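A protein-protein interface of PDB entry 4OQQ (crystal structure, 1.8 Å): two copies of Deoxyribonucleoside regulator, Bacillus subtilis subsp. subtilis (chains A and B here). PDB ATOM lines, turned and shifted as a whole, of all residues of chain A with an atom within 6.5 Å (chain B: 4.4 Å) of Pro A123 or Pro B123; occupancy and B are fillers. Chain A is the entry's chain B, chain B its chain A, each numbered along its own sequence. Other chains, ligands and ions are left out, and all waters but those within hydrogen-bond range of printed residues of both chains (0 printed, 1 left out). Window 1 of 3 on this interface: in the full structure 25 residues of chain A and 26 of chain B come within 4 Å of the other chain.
The backbone NH of Leu B124 sits close to the backbone carbonyl oxygen of Pro A123 (3.4 Å).
N of Pro A125 lies close to O of Pro B123 (3.3 Å).
The backbone carbonyl oxygen (O) of Tyr B121 lies within hydrogen-bond range of the side-chain hydroxyl (OG) of Ser A96, 2.7 Å away.
The backbone NH (N) of Leu A124 sits close to the backbone carbonyl oxygen (O) of Pro B123.
The backbone nitrogen (N) of Pro B125 sits close to the backbone carbonyl oxygen (O) of Pro A123, at 3.3 Å.
The backbone carbonyl oxygen of Pro A123 lies close to the backbone carbonyl oxygen of Pro B123, at 3.3 Å.
The backbone carbonyl oxygen of Leu A124 is in hydrogen-bond range of the backbone NH of Gly A94 (2.9 Å).
Among the printed residues, merely in contact across the chains: Ile A95 with Tyr B121 and Ser A96 with Ile B146.
Of chain B, only Pro B123 (3.3 Å), Leu B124 (3.1 Å) and Pro B125 (3.2 Å) come within 4 Å of Pro A123.
Of the printed residues of chain A, Pro B123 touches Pro A123, Leu A124 and Pro A125.
Of the printed residues of chain B, Ser A96 touches Tyr B121 and Ile B146.
Printed residues of chain A within 4 Å of Ile B146: Ser A96 (3.1 Å).
Of the printed residues of chain A, Pro B125 touches Pro A123 (3.2 Å).
Of the printed residues of chain B, Leu A124 touches Pro B123 (3.0 Å).
Of the printed residues of chain A, Leu B124 touches Pro A123.
The nearest printed residue of chain B that does not touch Pro A123 is Leu B122 (6.0 Å).
The nearest printed residue of chain A that does not touch Pro B123 is Ser A96 (4.3 Å).
Hydrophobic or aromatic side chains of chain B within 4 Å of the printed part of chain A: Tyr B121, Pro B123, Pro B125 and Ile B146.
Hydrophobic or aromatic side chains of chain A that line the printed part of chain B: Pro A123 and Pro A125.
Among the printed residues, no Asp or Glu carboxylate lies within 4 Å of a Lys or Arg side-chain nitrogen of the other chain.
Pro B123 touches its own counterpart, Pro A123.
Pro A123 touches Leu B124, and with the chains exchanged Leu A124 touches Pro B123.
Pro A123 touches Pro B125, and with the chains exchanged Pro A125 touches Pro B123.
Of the 8 pairs that touch across the chains among the printed residues, 5 have their exchanged pair printed and touching as well.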
ATOM      1  N   GLY A  94     -27.873  29.011  -6.077  1.00  0.00           N
ATOM      2  CA  GLY A  94     -29.148  29.674  -5.737  1.00  0.00           C
ATOM      3  C   GLY A  94     -29.016  31.173  -5.606  1.00  0.00           C
ATOM      4  O   GLY A  94     -27.906  31.699  -5.496  1.00  0.00           O
ATOM      5  N   ILE A  95     -30.138  31.894  -5.683  1.00  0.00           N
ATOM      6  CA  ILE A  95     -30.141  33.312  -5.440  1.00  0.00           C
ATOM      7  C   ILE A  95     -30.923  33.563  -4.161  1.00  0.00           C
ATOM      8  O   ILE A  95     -31.644  32.701  -3.649  1.00  0.00           O
ATOM      9  CB  ILE A  95     -30.757  34.140  -6.604  1.00  0.00           C
ATOM     10  CG1 ILE A  95     -32.242  33.737  -6.792  1.00  0.00           C
ATOM     11  CG2 ILE A  95     -29.909  33.951  -7.866  1.00  0.00           C
ATOM     12  CD1 ILE A  95     -33.003  34.697  -7.658  1.00  0.00           C
ATOM     13  N   SER A  96     -30.787  34.752  -3.620  1.00  0.00           N
ATOM     14  CA  SER A  96     -31.456  34.964  -2.362  1.00  0.00           C
ATOM     15  C   SER A  96     -32.769  35.675  -2.547  1.00  0.00           C
ATOM     16  O   SER A  96     -33.661  35.488  -1.730  1.00  0.00           O
ATOM     17  CB  SER A  96     -30.598  35.678  -1.334  1.00  0.00           C
ATOM     18  OG  SER A  96     -31.426  35.998  -0.217  1.00  0.00           O
ATOM     19  N   TYR A 121     -30.278  18.803  -3.643  1.00  0.00           N
ATOM     20  CA  TYR A 121     -30.127  20.246  -3.787  1.00  0.00           C
ATOM     21  C   TYR A 121     -28.662  20.644  -3.581  1.00  0.00           C
ATOM     22  O   TYR A 121     -27.891  19.912  -2.953  1.00  0.00           O
ATOM     23  CB  TYR A 121     -30.955  20.999  -2.757  1.00  0.00           C
ATOM     24  CG  TYR A 121     -32.426  20.709  -2.764  1.00  0.00           C
ATOM     25  CD1 TYR A 121     -33.275  21.303  -3.702  1.00  0.00           C
ATOM     26  CD2 TYR A 121     -32.982  19.852  -1.803  1.00  0.00           C
ATOM     27  CE1 TYR A 121     -34.640  21.016  -3.705  1.00  0.00           C
ATOM     28  CE2 TYR A 121     -34.331  19.573  -1.801  1.00  0.00           C
ATOM     29  CZ  TYR A 121     -35.147  20.163  -2.754  1.00  0.00           C
ATOM     30  OH  TYR A 121     -36.489  19.872  -2.717  1.00  0.00           O
ATOM     31  N   LEU A 122     -28.310  21.829  -4.092  1.00  0.00           N
ATOM     32  CA  LEU A 122     -27.009  22.452  -3.855  1.00  0.00           C
ATOM     33  C   LEU A 122     -27.315  23.730  -3.043  1.00  0.00           C
ATOM     34  O   LEU A 122     -27.629  24.740  -3.619  1.00  0.00           O
ATOM     35  CB  LEU A 122     -26.348  22.797  -5.163  1.00  0.00           C
ATOM     36  CG  LEU A 122     -24.975  23.480  -5.075  1.00  0.00           C
ATOM     37  CD1 LEU A 122     -23.983  22.530  -4.443  1.00  0.00           C
ATOM     38  CD2 LEU A 122     -24.550  23.889  -6.461  1.00  0.00           C
ATOM     39  N   PRO A 123     -27.266  23.659  -1.697  1.00  0.00           N
ATOM     40  CA  PRO A 123     -27.829  24.698  -0.841  1.00  0.00           C
ATOM     41  C   PRO A 123     -26.796  25.799  -0.603  1.00  0.00           C
ATOM     42  O   PRO A 123     -26.359  25.975   0.547  1.00  0.00           O
ATOM     43  CB  PRO A 123     -28.129  23.970   0.440  1.00  0.00           C
ATOM     44  CG  PRO A 123     -27.117  22.883   0.486  1.00  0.00           C
ATOM     45  CD  PRO A 123     -26.832  22.491  -0.933  1.00  0.00           C
ATOM     46  N   LEU A 124     -26.461  26.498  -1.662  1.00  0.00           N
ATOM     47  CA  LEU A 124     -25.428  27.547  -1.684  1.00  0.00           C
ATOM     48  C   LEU A 124     -25.851  28.690  -2.583  1.00  0.00           C
ATOM     49  O   LEU A 124     -26.674  28.509  -3.490  1.00  0.00           O
ATOM     50  CB  LEU A 124     -24.154  26.963  -2.237  1.00  0.00           C
ATOM     51  CG  LEU A 124     -23.418  25.942  -1.384  1.00  0.00           C
ATOM     52  CD1 LEU A 124     -22.212  25.434  -2.139  1.00  0.00           C
ATOM     53  CD2 LEU A 124     -23.008  26.528  -0.041  1.00  0.00           C
ATOM     54  N   PRO A 125     -25.256  29.889  -2.386  1.00  0.00           N
ATOM     55  CA  PRO A 125     -25.485  31.008  -3.272  1.00  0.00           C
ATOM     56  C   PRO A 125     -24.703  30.830  -4.532  1.00  0.00           C
ATOM     57  O   PRO A 125     -23.740  30.091  -4.576  1.00  0.00           O
ATOM     58  CB  PRO A 125     -24.947  32.209  -2.474  1.00  0.00           C
ATOM     59  CG  PRO A 125     -23.865  31.629  -1.632  1.00  0.00           C
ATOM     60  CD  PRO A 125     -24.376  30.258  -1.245  1.00  0.00           C
ATOM     61  N   VAL A 126     -25.108  31.510  -5.580  1.00  0.00           N
ATOM     62  CA  VAL A 126     -24.407  31.419  -6.827  1.00  0.00           C
ATOM     63  C   VAL A 126     -22.992  32.017  -6.768  1.00  0.00           C
ATOM     64  O   VAL A 126     -22.100  31.555  -7.471  1.00  0.00           O
ATOM     65  CB  VAL A 126     -25.246  32.016  -7.969  1.00  0.00           C
ATOM     66  CG1 VAL A 126     -25.682  33.450  -7.702  1.00  0.00           C
ATOM     67  CG2 VAL A 126     -24.472  31.966  -9.257  1.00  0.00           C
ATOM     68  N   PHE A 128     -20.006  33.992  -4.067  1.00  0.00           N
ATOM     69  CA  PHE A 128     -19.467  34.498  -2.831  1.00  0.00           C
ATOM     70  C   PHE A 128     -18.629  35.743  -3.122  1.00  0.00           C
ATOM     71  O   PHE A 128     -17.970  35.834  -4.167  1.00  0.00           O
ATOM     72  CB  PHE A 128     -18.576  33.436  -2.158  1.00  0.00           C
ATOM     73  CG  PHE A 128     -19.354  32.372  -1.436  1.00  0.00           C
ATOM     74  CD1 PHE A 128     -19.873  32.645  -0.178  1.00  0.00           C
ATOM     75  CD2 PHE A 128     -19.658  31.159  -2.037  1.00  0.00           C
ATOM     76  CE1 PHE A 128     -20.650  31.700   0.488  1.00  0.00           C
ATOM     77  CE2 PHE A 128     -20.389  30.183  -1.343  1.00  0.00           C
ATOM     78  CZ  PHE A 128     -20.926  30.484  -0.105  1.00  0.00           C
ATOM     79  N   ILE A 143     -20.800  19.525   1.474  1.00  0.00           N
ATOM     80  CA  ILE A 143     -20.893  20.167   0.159  1.00  0.00           C
ATOM     81  C   ILE A 143     -20.112  19.433  -0.925  1.00  0.00           C
ATOM     82  O   ILE A 143     -20.571  19.294  -2.040  1.00  0.00           O
ATOM     83  CB  ILE A 143     -20.450  21.650   0.208  1.00  0.00           C
ATOM     84  CG1 ILE A 143     -21.320  22.448   1.168  1.00  0.00           C
ATOM     85  CG2 ILE A 143     -20.355  22.248  -1.204  1.00  0.00           C
ATOM     86  CD1 ILE A 143     -22.800  22.618   0.804  1.00  0.00           C
ATOM     87  N   ILE A 146     -21.958  16.804  -2.760  1.00  0.00           N
ATOM     88  CA  ILE A 146     -22.934  17.307  -3.698  1.00  0.00           C
ATOM     89  C   ILE A 146     -22.229  17.707  -4.988  1.00  0.00           C
ATOM     90  O   ILE A 146     -22.696  17.423  -6.101  1.00  0.00           O
ATOM     91  CB  ILE A 146     -23.685  18.528  -3.127  1.00  0.00           C
ATOM     92  CG1 ILE A 146     -24.323  18.144  -1.793  1.00  0.00           C
ATOM     93  CG2 ILE A 146     -24.807  18.940  -4.062  1.00  0.00           C
ATOM     94  CD1 ILE A 146     -24.934  19.302  -1.018  1.00  0.00           C
ATOM     95  N   TYR A 174     -24.035  41.078  -7.022  1.00  0.00           N
ATOM     96  CA  TYR A 174     -22.849  40.283  -6.993  1.00  0.00           C
ATOM     97  C   TYR A 174     -21.627  40.919  -7.696  1.00  0.00           C
ATOM     98  O   TYR A 174     -20.482  40.544  -7.403  1.00  0.00           O
ATOM     99  CB  TYR A 174     -23.137  38.879  -7.560  1.00  0.00           C
ATOM    100  CG  TYR A 174     -24.048  38.008  -6.712  1.00  0.00           C
ATOM    101  CD1 TYR A 174     -23.728  37.732  -5.399  1.00  0.00           C
ATOM    102  CD2 TYR A 174     -25.197  37.419  -7.240  1.00  0.00           C
ATOM    103  CE1 TYR A 174     -24.518  36.895  -4.627  1.00  0.00           C
ATOM    104  CE2 TYR A 174     -26.018  36.610  -6.475  1.00  0.00           C
ATOM    105  CZ  TYR A 174     -25.678  36.347  -5.156  1.00  0.00           C
ATOM    106  OH  TYR A 174     -26.415  35.501  -4.329  1.00  0.00           O
ATOM    107  N   TYR B 121     -34.666  34.162   0.470  1.00  0.00           N
ATOM    108  CA  TYR B 121     -34.189  32.835   0.841  1.00  0.00           C
ATOM    109  C   TYR B 121     -32.875  32.979   1.597  1.00  0.00           C
ATOM    110  O   TYR B 121     -32.221  34.039   1.540  1.00  0.00           O
ATOM    111  CB  TYR B 121     -33.948  31.965  -0.376  1.00  0.00           C
ATOM    112  CG  TYR B 121     -35.121  31.764  -1.288  1.00  0.00           C
ATOM    113  CD1 TYR B 121     -36.101  30.841  -0.991  1.00  0.00           C
ATOM    114  CD2 TYR B 121     -35.223  32.483  -2.491  1.00  0.00           C
ATOM    115  CE1 TYR B 121     -37.176  30.640  -1.847  1.00  0.00           C
ATOM    116  CE2 TYR B 121     -36.285  32.291  -3.343  1.00  0.00           C
ATOM    117  CZ  TYR B 121     -37.255  31.366  -3.011  1.00  0.00           C
ATOM    118  OH  TYR B 121     -38.314  31.184  -3.866  1.00  0.00           O
ATOM    119  N   LEU B 122     -32.510  31.911   2.326  1.00  0.00           N
ATOM    120  CA  LEU B 122     -31.230  31.801   3.031  1.00  0.00           C
ATOM    121  C   LEU B 122     -30.532  30.605   2.350  1.00  0.00           C
ATOM    122  O   LEU B 122     -30.796  29.461   2.708  1.00  0.00           O
ATOM    123  CB  LEU B 122     -31.461  31.533   4.512  1.00  0.00           C
ATOM    124  CG  LEU B 122     -30.212  31.337   5.388  1.00  0.00           C
ATOM    125  CD1 LEU B 122     -29.307  32.527   5.304  1.00  0.00           C
ATOM    126  CD2 LEU B 122     -30.629  31.094   6.824  1.00  0.00           C
ATOM    127  N   PRO B 123     -29.718  30.859   1.296  1.00  0.00           N
ATOM    128  CA  PRO B 123     -29.252  29.775   0.419  1.00  0.00           C
ATOM    129  C   PRO B 123     -27.974  29.122   0.978  1.00  0.00           C
ATOM    130  O   PRO B 123     -26.899  29.258   0.368  1.00  0.00           O
ATOM    131  CB  PRO B 123     -28.963  30.494  -0.885  1.00  0.00           C
ATOM    132  CG  PRO B 123     -28.562  31.861  -0.465  1.00  0.00           C
ATOM    133  CD  PRO B 123     -29.340  32.177   0.792  1.00  0.00           C
ATOM    134  N   LEU B 124     -28.134  28.424   2.096  1.00  0.00           N
ATOM    135  CA  LEU B 124     -27.043  27.833   2.882  1.00  0.00           C
ATOM    136  C   LEU B 124     -27.524  26.499   3.459  1.00  0.00           C
ATOM    137  O   LEU B 124     -28.735  26.273   3.563  1.00  0.00           O
ATOM    138  CB  LEU B 124     -26.693  28.750   4.034  1.00  0.00           C
ATOM    139  CG  LEU B 124     -25.965  30.037   3.692  1.00  0.00           C
ATOM    140  CD1 LEU B 124     -25.654  30.816   4.961  1.00  0.00           C
ATOM    141  CD2 LEU B 124     -24.717  29.806   2.853  1.00  0.00           C
ATOM    142  N   PRO B 125     -26.599  25.603   3.779  1.00  0.00           N
ATOM    143  CA  PRO B 125     -26.930  24.371   4.482  1.00  0.00           C
ATOM    144  C   PRO B 125     -27.186  24.663   5.937  1.00  0.00           C
ATOM    145  O   PRO B 125     -26.735  25.656   6.473  1.00  0.00           O
ATOM    146  CB  PRO B 125     -25.659  23.523   4.299  1.00  0.00           C
ATOM    147  CG  PRO B 125     -24.571  24.540   4.233  1.00  0.00           C
ATOM    148  CD  PRO B 125     -25.162  25.684   3.466  1.00  0.00           C
ATOM    149  N   ILE B 143     -24.501  37.236   2.205  1.00  0.00           N
ATOM    150  CA  ILE B 143     -25.125  36.447   3.280  1.00  0.00           C
ATOM    151  C   ILE B 143     -25.435  37.258   4.544  1.00  0.00           C
ATOM    152  O   ILE B 143     -26.470  37.105   5.148  1.00  0.00           O
ATOM    153  CB  ILE B 143     -24.267  35.222   3.660  1.00  0.00           C
ATOM    154  CG1 ILE B 143     -24.067  34.284   2.470  1.00  0.00           C
ATOM    155  CG2 ILE B 143     -24.841  34.503   4.900  1.00  0.00           C
ATOM    156  CD1 ILE B 143     -25.313  33.649   1.850  1.00  0.00           C
ATOM    157  N   ILE B 146     -28.730  38.884   4.595  1.00  0.00           N
ATOM    158  CA  ILE B 146     -29.852  38.005   4.791  1.00  0.00           C
ATOM    159  C   ILE B 146     -29.998  37.732   6.275  1.00  0.00           C
ATOM    160  O   ILE B 146     -31.099  37.758   6.856  1.00  0.00           O
ATOM    161  CB  ILE B 146     -29.670  36.676   4.023  1.00  0.00           C
ATOM    162  CG1 ILE B 146     -29.452  36.951   2.532  1.00  0.00           C
ATOM    163  CG2 ILE B 146     -30.925  35.819   4.109  1.00  0.00           C
ATOM    164  CD1 ILE B 146     -29.068  35.756   1.706  1.00  0.00           C
